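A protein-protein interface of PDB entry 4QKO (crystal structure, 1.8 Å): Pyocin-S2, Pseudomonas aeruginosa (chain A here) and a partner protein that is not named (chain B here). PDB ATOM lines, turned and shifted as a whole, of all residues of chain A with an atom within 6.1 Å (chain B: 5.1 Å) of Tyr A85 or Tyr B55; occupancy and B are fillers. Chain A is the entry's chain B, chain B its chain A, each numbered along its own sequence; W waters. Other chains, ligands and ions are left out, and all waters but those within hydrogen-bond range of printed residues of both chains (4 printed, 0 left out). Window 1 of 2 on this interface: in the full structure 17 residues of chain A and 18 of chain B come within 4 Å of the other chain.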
ATOM      1  N   ASN A  71     -18.720  -1.842  -0.159  1.00  0.00           N
ATOM      2  CA  ASN A  71     -18.307  -1.103   0.990  1.00  0.00           C
ATOM      3  C   ASN A  71     -18.271   0.385   0.724  1.00  0.00           C
ATOM      4  O   ASN A  71     -18.444   0.825  -0.401  1.00  0.00           O
ATOM      5  CB  ASN A  71     -16.965  -1.647   1.556  1.00  0.00           C
ATOM      6  CG  ASN A  71     -15.749  -1.007   0.943  1.00  0.00           C
ATOM      7  OD1 ASN A  71     -15.739  -0.703  -0.216  1.00  0.00           O
ATOM      8  ND2 ASN A  71     -14.684  -0.812   1.757  1.00  0.00           N
ATOM      9  N   GLY A  73     -15.929   2.551   0.540  1.00  0.00           N
ATOM     10  CA  GLY A  73     -14.922   2.921  -0.430  1.00  0.00           C
ATOM     11  C   GLY A  73     -15.440   2.724  -1.830  1.00  0.00           C
ATOM     12  O   GLY A  73     -15.246   3.554  -2.719  1.00  0.00           O
ATOM     13  N   SER A  74     -16.044   1.578  -2.080  1.00  0.00           N
ATOM     14  CA  SER A  74     -16.532   1.300  -3.413  1.00  0.00           C
ATOM     15  C   SER A  74     -17.703   2.220  -3.814  1.00  0.00           C
ATOM     16  O   SER A  74     -17.797   2.674  -4.966  1.00  0.00           O
ATOM     17  CB  SER A  74     -16.986  -0.146  -3.464  1.00  0.00           C
ATOM     18  OG  SER A  74     -15.894  -1.056  -3.512  1.00  0.00           O
ATOM     19  N   VAL A  77     -16.803   5.558  -5.186  1.00  0.00           N
ATOM     20  CA  VAL A  77     -16.394   5.519  -6.573  1.00  0.00           C
ATOM     21  C   VAL A  77     -17.647   5.400  -7.472  1.00  0.00           C
ATOM     22  O   VAL A  77     -17.757   6.128  -8.470  1.00  0.00           O
ATOM     23  CB  VAL A  77     -15.417   4.334  -6.815  1.00  0.00           C
ATOM     24  CG1 VAL A  77     -15.296   4.034  -8.291  1.00  0.00           C
ATOM     25  CG2 VAL A  77     -14.057   4.676  -6.216  1.00  0.00           C
ATOM     26  N   ALA A  83     -16.827   2.410 -12.115  1.00  0.00           N
ATOM     27  CA  ALA A  83     -16.978   1.001 -11.803  1.00  0.00           C
ATOM     28  C   ALA A  83     -16.185   0.684 -10.549  1.00  0.00           C
ATOM     29  O   ALA A  83     -15.124   1.229 -10.338  1.00  0.00           O
ATOM     30  CB  ALA A  83     -16.431   0.140 -12.943  1.00  0.00           C
ATOM     31  N   PRO A  84     -16.612  -0.344  -9.807  1.00  0.00           N
ATOM     32  CA  PRO A  84     -15.866  -0.747  -8.658  1.00  0.00           C
ATOM     33  C   PRO A  84     -14.583  -1.424  -9.048  1.00  0.00           C
ATOM     34  O   PRO A  84     -14.473  -2.061 -10.107  1.00  0.00           O
ATOM     35  CB  PRO A  84     -16.771  -1.743  -7.964  1.00  0.00           C
ATOM     36  CG  PRO A  84     -17.736  -2.207  -9.013  1.00  0.00           C
ATOM     37  CD  PRO A  84     -17.825  -1.142 -10.033  1.00  0.00           C
ATOM     38  N   TYR A  85     -13.637  -1.332  -8.128  1.00  0.00           N
ATOM     39  CA  TYR A  85     -12.416  -2.144  -8.226  1.00  0.00           C
ATOM     40  C   TYR A  85     -12.702  -3.630  -7.907  1.00  0.00           C
ATOM     41  O   TYR A  85     -13.558  -3.942  -7.059  1.00  0.00           O
ATOM     42  CB  TYR A  85     -11.316  -1.614  -7.242  1.00  0.00           C
ATOM     43  CG  TYR A  85     -10.777  -0.242  -7.636  1.00  0.00           C
ATOM     44  CD1 TYR A  85     -11.452   0.938  -7.230  1.00  0.00           C
ATOM     45  CD2 TYR A  85      -9.705  -0.109  -8.415  1.00  0.00           C
ATOM     46  CE1 TYR A  85     -10.976   2.190  -7.573  1.00  0.00           C
ATOM     47  CE2 TYR A  85      -9.189   1.123  -8.744  1.00  0.00           C
ATOM     48  CZ  TYR A  85      -9.852   2.284  -8.351  1.00  0.00           C
ATOM     49  OH  TYR A  85      -9.378   3.544  -8.706  1.00  0.00           O
ATOM     50  N   VAL A  86     -12.083  -4.552  -8.672  1.00  0.00           N
ATOM     51  CA  VAL A  86     -12.181  -5.966  -8.351  1.00  0.00           C
ATOM     52  C   VAL A  86     -11.164  -6.374  -7.278  1.00  0.00           C
ATOM     53  O   VAL A  86     -10.239  -5.638  -6.889  1.00  0.00           O
ATOM     54  CB  VAL A  86     -12.082  -6.900  -9.578  1.00  0.00           C
ATOM     55  CG1 VAL A  86     -13.150  -6.496 -10.582  1.00  0.00           C
ATOM     56  CG2 VAL A  86     -10.699  -6.796 -10.223  1.00  0.00           C
ATOM     57  N   ARG A  87     -11.396  -7.532  -6.765  1.00  0.00           N
ATOM     58  CA  ARG A  87     -10.464  -8.169  -5.830  1.00  0.00           C
ATOM     59  C   ARG A  87      -9.133  -8.347  -6.501  1.00  0.00           C
ATOM     60  O   ARG A  87      -9.056  -8.554  -7.714  1.00  0.00           O
ATOM     61  CB  ARG A  87     -10.995  -9.511  -5.367  1.00  0.00           C
ATOM     62  CG  ARG A  87     -12.157  -9.419  -4.403  1.00  0.00           C
ATOM     63  CD  ARG A  87     -12.809 -10.787  -4.255  1.00  0.00           C
ATOM     64  NE  ARG A  87     -13.934 -10.707  -3.310  1.00  0.00           N
ATOM     65  CZ  ARG A  87     -13.807 -10.701  -1.991  1.00  0.00           C
ATOM     66  NH1 ARG A  87     -12.630 -10.852  -1.381  1.00  0.00           N
ATOM     67  NH2 ARG A  87     -14.901 -10.550  -1.250  1.00  0.00           N
ATOM     68  N   GLN A  91      -7.703  -9.100 -10.759  1.00  0.00           N
ATOM     69  CA  GLN A  91      -7.008  -8.074 -11.527  1.00  0.00           C
ATOM     70  C   GLN A  91      -6.118  -8.808 -12.589  1.00  0.00           C
ATOM     71  O   GLN A  91      -5.639  -9.935 -12.379  1.00  0.00           O
ATOM     72  CB  GLN A  91      -6.151  -7.187 -10.625  1.00  0.00           C
ATOM     73  CG  GLN A  91      -7.052  -6.511  -9.538  1.00  0.00           C
ATOM     74  CD  GLN A  91      -6.351  -5.547  -8.625  1.00  0.00           C
ATOM     75  OE1 GLN A  91      -5.174  -5.348  -8.739  1.00  0.00           O
ATOM     76  NE2 GLN A  91      -7.075  -4.985  -7.675  1.00  0.00           N
ATOM     77  N   ILE A  96      -8.165  -3.283 -13.422  1.00  0.00           N
ATOM     78  CA  ILE A  96      -8.444  -3.480 -12.044  1.00  0.00           C
ATOM     79  C   ILE A  96      -9.918  -3.184 -11.666  1.00  0.00           C
ATOM     80  O   ILE A  96     -10.244  -3.248 -10.533  1.00  0.00           O
ATOM     81  CB  ILE A  96      -7.397  -2.724 -11.124  1.00  0.00           C
ATOM     82  CG1 ILE A  96      -7.470  -1.213 -11.302  1.00  0.00           C
ATOM     83  CG2 ILE A  96      -5.979  -3.175 -11.504  1.00  0.00           C
ATOM     84  CD1 ILE A  96      -6.641  -0.452 -10.287  1.00  0.00           C
ATOM     85  N   LYS A  97     -10.785  -2.953 -12.648  1.00  0.00           N
ATOM     86  CA  LYS A  97     -12.194  -2.619 -12.426  1.00  0.00           C
ATOM     87  C   LYS A  97     -13.113  -3.593 -13.163  1.00  0.00           C
ATOM     88  O   LYS A  97     -12.701  -4.240 -14.144  1.00  0.00           O
ATOM     89  CB  LYS A  97     -12.472  -1.187 -12.863  1.00  0.00           C
ATOM     90  CG  LYS A  97     -12.049  -0.272 -11.761  1.00  0.00           C
ATOM     91  CD  LYS A  97     -12.019   1.128 -12.218  1.00  0.00           C
ATOM     92  CE  LYS A  97     -11.919   2.058 -11.026  1.00  0.00           C
ATOM     93  NZ  LYS A  97     -13.020   3.035 -11.132  1.00  0.00           N
ATOM     94  N   ILE A  98     -14.309  -3.757 -12.634  1.00  0.00           N
ATOM     95  CA  ILE A  98     -15.359  -4.485 -13.301  1.00  0.00           C
ATOM     96  C   ILE A  98     -15.596  -3.867 -14.701  1.00  0.00           C
ATOM     97  O   ILE A  98     -15.681  -2.592 -14.892  1.00  0.00           O
ATOM     98  CB  ILE A  98     -16.666  -4.459 -12.515  1.00  0.00           C
ATOM     99  CG1 ILE A  98     -16.643  -5.297 -11.196  1.00  0.00           C
ATOM    100  CG2 ILE A  98     -17.807  -4.957 -13.348  1.00  0.00           C
ATOM    101  CD1 ILE A  98     -16.585  -6.816 -11.380  1.00  0.00           C
ATOM    102  N   ILE B  20      -8.310   8.756  -1.117  1.00  0.00           N
ATOM    103  CA  ILE B  20      -8.655   7.643  -2.022  1.00  0.00           C
ATOM    104  C   ILE B  20     -10.002   7.023  -1.638  1.00  0.00           C
ATOM    105  O   ILE B  20     -10.880   6.849  -2.497  1.00  0.00           O
ATOM    106  CB  ILE B  20      -7.583   6.522  -1.984  1.00  0.00           C
ATOM    107  CG1 ILE B  20      -6.287   7.068  -2.528  1.00  0.00           C
ATOM    108  CG2 ILE B  20      -8.079   5.328  -2.769  1.00  0.00           C
ATOM    109  CD1 ILE B  20      -5.090   6.124  -2.501  1.00  0.00           C
ATOM    110  N   GLU B  31     -11.461   9.671 -13.046  1.00  0.00           N
ATOM    111  CA  GLU B  31     -11.395   8.263 -12.723  1.00  0.00           C
ATOM    112  C   GLU B  31      -9.972   7.749 -12.931  1.00  0.00           C
ATOM    113  O   GLU B  31      -9.449   6.945 -12.119  1.00  0.00           O
ATOM    114  CB  GLU B  31     -12.423   7.426 -13.530  1.00  0.00           C
ATOM    115  CG  GLU B  31     -12.482   5.980 -13.088  1.00  0.00           C
ATOM    116  CD  GLU B  31     -13.560   5.149 -13.777  1.00  0.00           C
ATOM    117  OE1 GLU B  31     -14.293   5.672 -14.643  1.00  0.00           O
ATOM    118  OE2 GLU B  31     -13.666   3.943 -13.485  1.00  0.00           O
ATOM    119  N   HIS B  34      -7.809   8.700 -10.021  1.00  0.00           N
ATOM    120  CA  HIS B  34      -8.053   7.828  -8.875  1.00  0.00           C
ATOM    121  C   HIS B  34      -7.367   6.476  -9.049  1.00  0.00           C
ATOM    122  O   HIS B  34      -6.831   5.910  -8.082  1.00  0.00           O
ATOM    123  CB  HIS B  34      -9.569   7.609  -8.697  1.00  0.00           C
ATOM    124  CG  HIS B  34      -9.940   7.047  -7.386  1.00  0.00           C
ATOM    125  ND1 HIS B  34     -10.065   5.686  -7.189  1.00  0.00           N
ATOM    126  CD2 HIS B  34     -10.227   7.634  -6.202  1.00  0.00           C
ATOM    127  CE1 HIS B  34     -10.410   5.466  -5.935  1.00  0.00           C
ATOM    128  NE2 HIS B  34     -10.525   6.632  -5.309  1.00  0.00           N
ATOM    129  N   ILE B  35      -7.427   5.926 -10.243  1.00  0.00           N
ATOM    130  CA  ILE B  35      -6.804   4.640 -10.488  1.00  0.00           C
ATOM    131  C   ILE B  35      -5.322   4.720 -10.200  1.00  0.00           C
ATOM    132  O   ILE B  35      -4.737   3.802  -9.575  1.00  0.00           O
ATOM    133  CB  ILE B  35      -7.068   4.106 -11.918  1.00  0.00           C
ATOM    134  CG1 ILE B  35      -8.525   3.671 -12.085  1.00  0.00           C
ATOM    135  CG2 ILE B  35      -6.159   2.907 -12.217  1.00  0.00           C
ATOM    136  CD1 ILE B  35      -9.018   3.465 -13.508  1.00  0.00           C
ATOM    137  N   VAL B  38      -4.704   4.646  -6.425  1.00  0.00           N
ATOM    138  CA  VAL B  38      -4.822   3.272  -5.958  1.00  0.00           C
ATOM    139  C   VAL B  38      -3.534   2.456  -6.281  1.00  0.00           C
ATOM    140  O   VAL B  38      -3.019   1.768  -5.410  1.00  0.00           O
ATOM    141  CB  VAL B  38      -6.049   2.593  -6.488  1.00  0.00           C
ATOM    142  CG1 VAL B  38      -6.038   1.099  -6.121  1.00  0.00           C
ATOM    143  CG2 VAL B  38      -7.277   3.202  -5.856  1.00  0.00           C
ATOM    144  N   SER B  51      -5.067  -3.451  -3.091  1.00  0.00           N
ATOM    145  CA  SER B  51      -6.301  -2.618  -3.043  1.00  0.00           C
ATOM    146  C   SER B  51      -7.405  -3.281  -2.199  1.00  0.00           C
ATOM    147  O   SER B  51      -8.394  -2.632  -1.853  1.00  0.00           O
ATOM    148  CB  SER B  51      -6.810  -2.286  -4.437  1.00  0.00           C
ATOM    149  OG  SER B  51      -7.052  -3.392  -5.257  1.00  0.00           O
ATOM    150  N   ASP B  52      -7.273  -4.581  -1.852  1.00  0.00           N
ATOM    151  CA  ASP B  52      -8.317  -5.211  -1.082  1.00  0.00           C
ATOM    152  C   ASP B  52      -8.371  -4.571   0.292  1.00  0.00           C
ATOM    153  O   ASP B  52      -9.394  -4.631   0.890  1.00  0.00           O
ATOM    154  CB  ASP B  52      -8.195  -6.715  -0.865  1.00  0.00           C
ATOM    155  CG  ASP B  52      -8.336  -7.529  -2.132  1.00  0.00           C
ATOM    156  OD1 ASP B  52      -8.673  -6.981  -3.189  1.00  0.00           O
ATOM    157  OD2 ASP B  52      -8.106  -8.806  -2.061  1.00  0.00           O
ATOM    158  N   LEU B  53      -7.286  -3.929   0.766  1.00  0.00           N
ATOM    159  CA  LEU B  53      -7.274  -3.196   2.047  1.00  0.00           C
ATOM    160  C   LEU B  53      -8.357  -2.128   2.019  1.00  0.00           C
ATOM    161  O   LEU B  53      -8.970  -1.897   3.018  1.00  0.00           O
ATOM    162  CB  LEU B  53      -5.935  -2.520   2.259  1.00  0.00           C
ATOM    163  CG  LEU B  53      -4.746  -3.436   2.515  1.00  0.00           C
ATOM    164  CD1 LEU B  53      -3.512  -2.613   2.739  1.00  0.00           C
ATOM    165  CD2 LEU B  53      -4.971  -4.281   3.755  1.00  0.00           C
ATOM    166  N   LEU B  54      -8.530  -1.513   0.840  1.00  0.00           N
ATOM    167  CA  LEU B  54      -9.521  -0.478   0.719  1.00  0.00           C
ATOM    168  C   LEU B  54     -10.920  -0.976   0.471  1.00  0.00           C
ATOM    169  O   LEU B  54     -11.868  -0.444   1.014  1.00  0.00           O
ATOM    170  CB  LEU B  54      -9.135   0.402  -0.478  1.00  0.00           C
ATOM    171  CG  LEU B  54      -7.777   1.113  -0.490  1.00  0.00           C
ATOM    172  CD1 LEU B  54      -7.516   1.648  -1.844  1.00  0.00           C
ATOM    173  CD2 LEU B  54      -7.786   2.261   0.482  1.00  0.00           C
ATOM    174  N   TYR B  55     -11.074  -1.955  -0.415  1.00  0.00           N
ATOM    175  CA  TYR B  55     -12.372  -2.381  -0.933  1.00  0.00           C
ATOM    176  C   TYR B  55     -12.935  -3.704  -0.468  1.00  0.00           C
ATOM    177  O   TYR B  55     -14.141  -3.920  -0.537  1.00  0.00           O
ATOM    178  CB  TYR B  55     -12.381  -2.311  -2.445  1.00  0.00           C
ATOM    179  CG  TYR B  55     -12.005  -0.909  -2.910  1.00  0.00           C
ATOM    180  CD1 TYR B  55     -12.783   0.181  -2.580  1.00  0.00           C
ATOM    181  CD2 TYR B  55     -10.826  -0.669  -3.536  1.00  0.00           C
ATOM    182  CE1 TYR B  55     -12.410   1.482  -2.959  1.00  0.00           C
ATOM    183  CE2 TYR B  55     -10.467   0.612  -3.969  1.00  0.00           C
ATOM    184  CZ  TYR B  55     -11.247   1.680  -3.650  1.00  0.00           C
ATOM    185  OH  TYR B  55     -10.843   2.960  -3.956  1.00  0.00           O
ATOM    186  N   TYR B  56     -12.085  -4.590   0.002  1.00  0.00           N
ATOM    187  CA  TYR B  56     -12.509  -5.886   0.409  1.00  0.00           C
ATOM    188  C   TYR B  56     -11.790  -6.216   1.715  1.00  0.00           C
ATOM    189  O   TYR B  56     -10.984  -7.204   1.808  1.00  0.00           O
ATOM    190  CB  TYR B  56     -12.201  -6.948  -0.678  1.00  0.00           C
ATOM    191  CG  TYR B  56     -12.870  -6.639  -1.972  1.00  0.00           C
ATOM    192  CD1 TYR B  56     -14.147  -7.061  -2.212  1.00  0.00           C
ATOM    193  CD2 TYR B  56     -12.198  -5.904  -2.931  1.00  0.00           C
ATOM    194  CE1 TYR B  56     -14.779  -6.765  -3.436  1.00  0.00           C
ATOM    195  CE2 TYR B  56     -12.779  -5.595  -4.144  1.00  0.00           C
ATOM    196  CZ  TYR B  56     -14.107  -6.009  -4.356  1.00  0.00           C
ATOM    197  OH  TYR B  56     -14.742  -5.697  -5.515  1.00  0.00           O
ATOM    198  N   PRO B  57     -11.973  -5.364   2.723  1.00  0.00           N
ATOM    199  CA  PRO B  57     -11.125  -5.412   3.912  1.00  0.00           C
ATOM    200  C   PRO B  57     -11.442  -6.636   4.772  1.00  0.00           C
ATOM    201  O   PRO B  57     -12.564  -7.200   4.746  1.00  0.00           O
ATOM    202  CB  PRO B  57     -11.515  -4.128   4.636  1.00  0.00           C
ATOM    203  CG  PRO B  57     -12.914  -3.976   4.216  1.00  0.00           C
ATOM    204  CD  PRO B  57     -12.884  -4.232   2.777  1.00  0.00           C
HETATM  205  O   HOH W   1     -12.631   4.794  -3.182  1.00  0.00           O
HETATM  206  O   HOH W   2     -16.554  -3.237  -1.929  1.00  0.00           O
HETATM  207  O   HOH W   3     -12.026   5.159  -9.720  1.00  0.00           O
HETATM  208  O   HOH W   4      -9.170  -4.700  -4.533  1.00  0.00           O
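NZ of Lys A97 is in salt-bridge range of OE2 of Glu B31 (2.6 Å).
OH of Tyr A85 sits at hydrogen-bond distance from ND1 of His B34 (2.7 Å).
N of Ile B35 lies close to OH of Tyr A85, 3.4 Å away.
The side-chain hydroxyl (OG) of Ser B51 lies within hydrogen-bond range of the side-chain amide nitrogen (NE2) of Gln A91 (2.9 Å).
The backbone carbonyl oxygen (O) of Leu B54 is in hydrogen-bond range of the side-chain amide nitrogen (ND2) of Asn A71, at 2.9 Å.
O of Tyr A85 sits at hydrogen-bond distance from OH of Tyr B56 (2.6 Å).
The backbone carbonyl oxygen of Ile B20 lies within hydrogen-bond range of a ring nitrogen (NE2) of His B34, 2.8 Å away.
The side-chain amide oxygen (OD1) of Asn A71 sits close to the backbone NH (N) of Gly A73.
The side-chain amide oxygen (OD1) of Asn A71 sits at hydrogen-bond distance from the backbone NH (N) of Ser A74, at 3.0 Å.
The side-chain amino group of Lys A97 is in hydrogen-bond range of the backbone carbonyl oxygen of Ala A83.
The backbone carbonyl oxygen (O) of Val A86 is in hydrogen-bond range of the side-chain amide nitrogen (NE2) of Gln A91.
The backbone NH (N) of Val A86 sits at hydrogen-bond distance from the backbone carbonyl oxygen (O) of Ile A96 (2.9 Å).
Tyr B55 touches Asn A71.
Asn A71 touches Pro B57 (ND2 to CD, 3.997 Å).
His B34 touches Val A77.
Glu B31 touches Ala A83 (OE2 to N, 3.8 Å).
Val B38 touches Tyr A85.
Val A86 touches Tyr B56 (C to CE2, 3.6 Å).
Asp B52 touches Arg A87 (OD1 to CA, 3.4 Å).
N of Arg A87 touches CE2 of Tyr B56 (3.5 Å).
Ile A96 touches Ile B35.
Lys A97 touches Ile B35.
Printed residues of chain B within 4 Å of Tyr A85: His B34, Ile B35, Val B38, Tyr B55 and Tyr B56.
Printed residues of chain A within 4 Å of Pro B57: Asn A71.
Printed residues of chain B within 4 Å of Val A86: Tyr B56 (3.6 Å).
Of the printed residues of chain A, His B34 touches Val A77 and Tyr A85.
Printed residues of chain B within 4 Å of Asn A71: Leu B54, Tyr B55 and Pro B57.
Of the printed residues of chain A, Ser B51 touches Gln A91.
Ile B20 touches none of the printed residues of chain A.
The nearest residue of chain A that does not touch Tyr B55 is Val A77 (4.3 Å).
Of the 12 printed residues of chain B, 10 touch a printed residue of chain A.
Hydrophobic or aromatic side chains of chain B within 4 Å of the printed part of chain A: His B34, Ile B35, Val B38, Tyr B55, Tyr B56 and Pro B57.
Of the 13 printed residues of chain A, 11 touch a printed residue of chain B.
Among the printed residues, 19 pairs touch across the chains.
Water W4 lies within hydrogen-bond range of OG of Ser B51 (2.6 Å), OD1 of Asp B52 (2.7 Å) and O of Val A86 (2.8 Å).
Water W1 lies within hydrogen-bond range of OH of Tyr B55 (2.7 Å), O of Ile B20 (2.8 Å) and O of Gly A73 (2.9 Å).
Water W3 lies within hydrogen-bond range of NZ of Lys A97 (2.7 Å), ND1 of His B34 (3.2 Å) and OH of Tyr A85 (3.3 Å).
Water W2 lies within hydrogen-bond range of OG of Ser A74 (2.8 Å), O of Tyr B55 (2.9 Å) and N of Asn A71 (3.1 Å).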
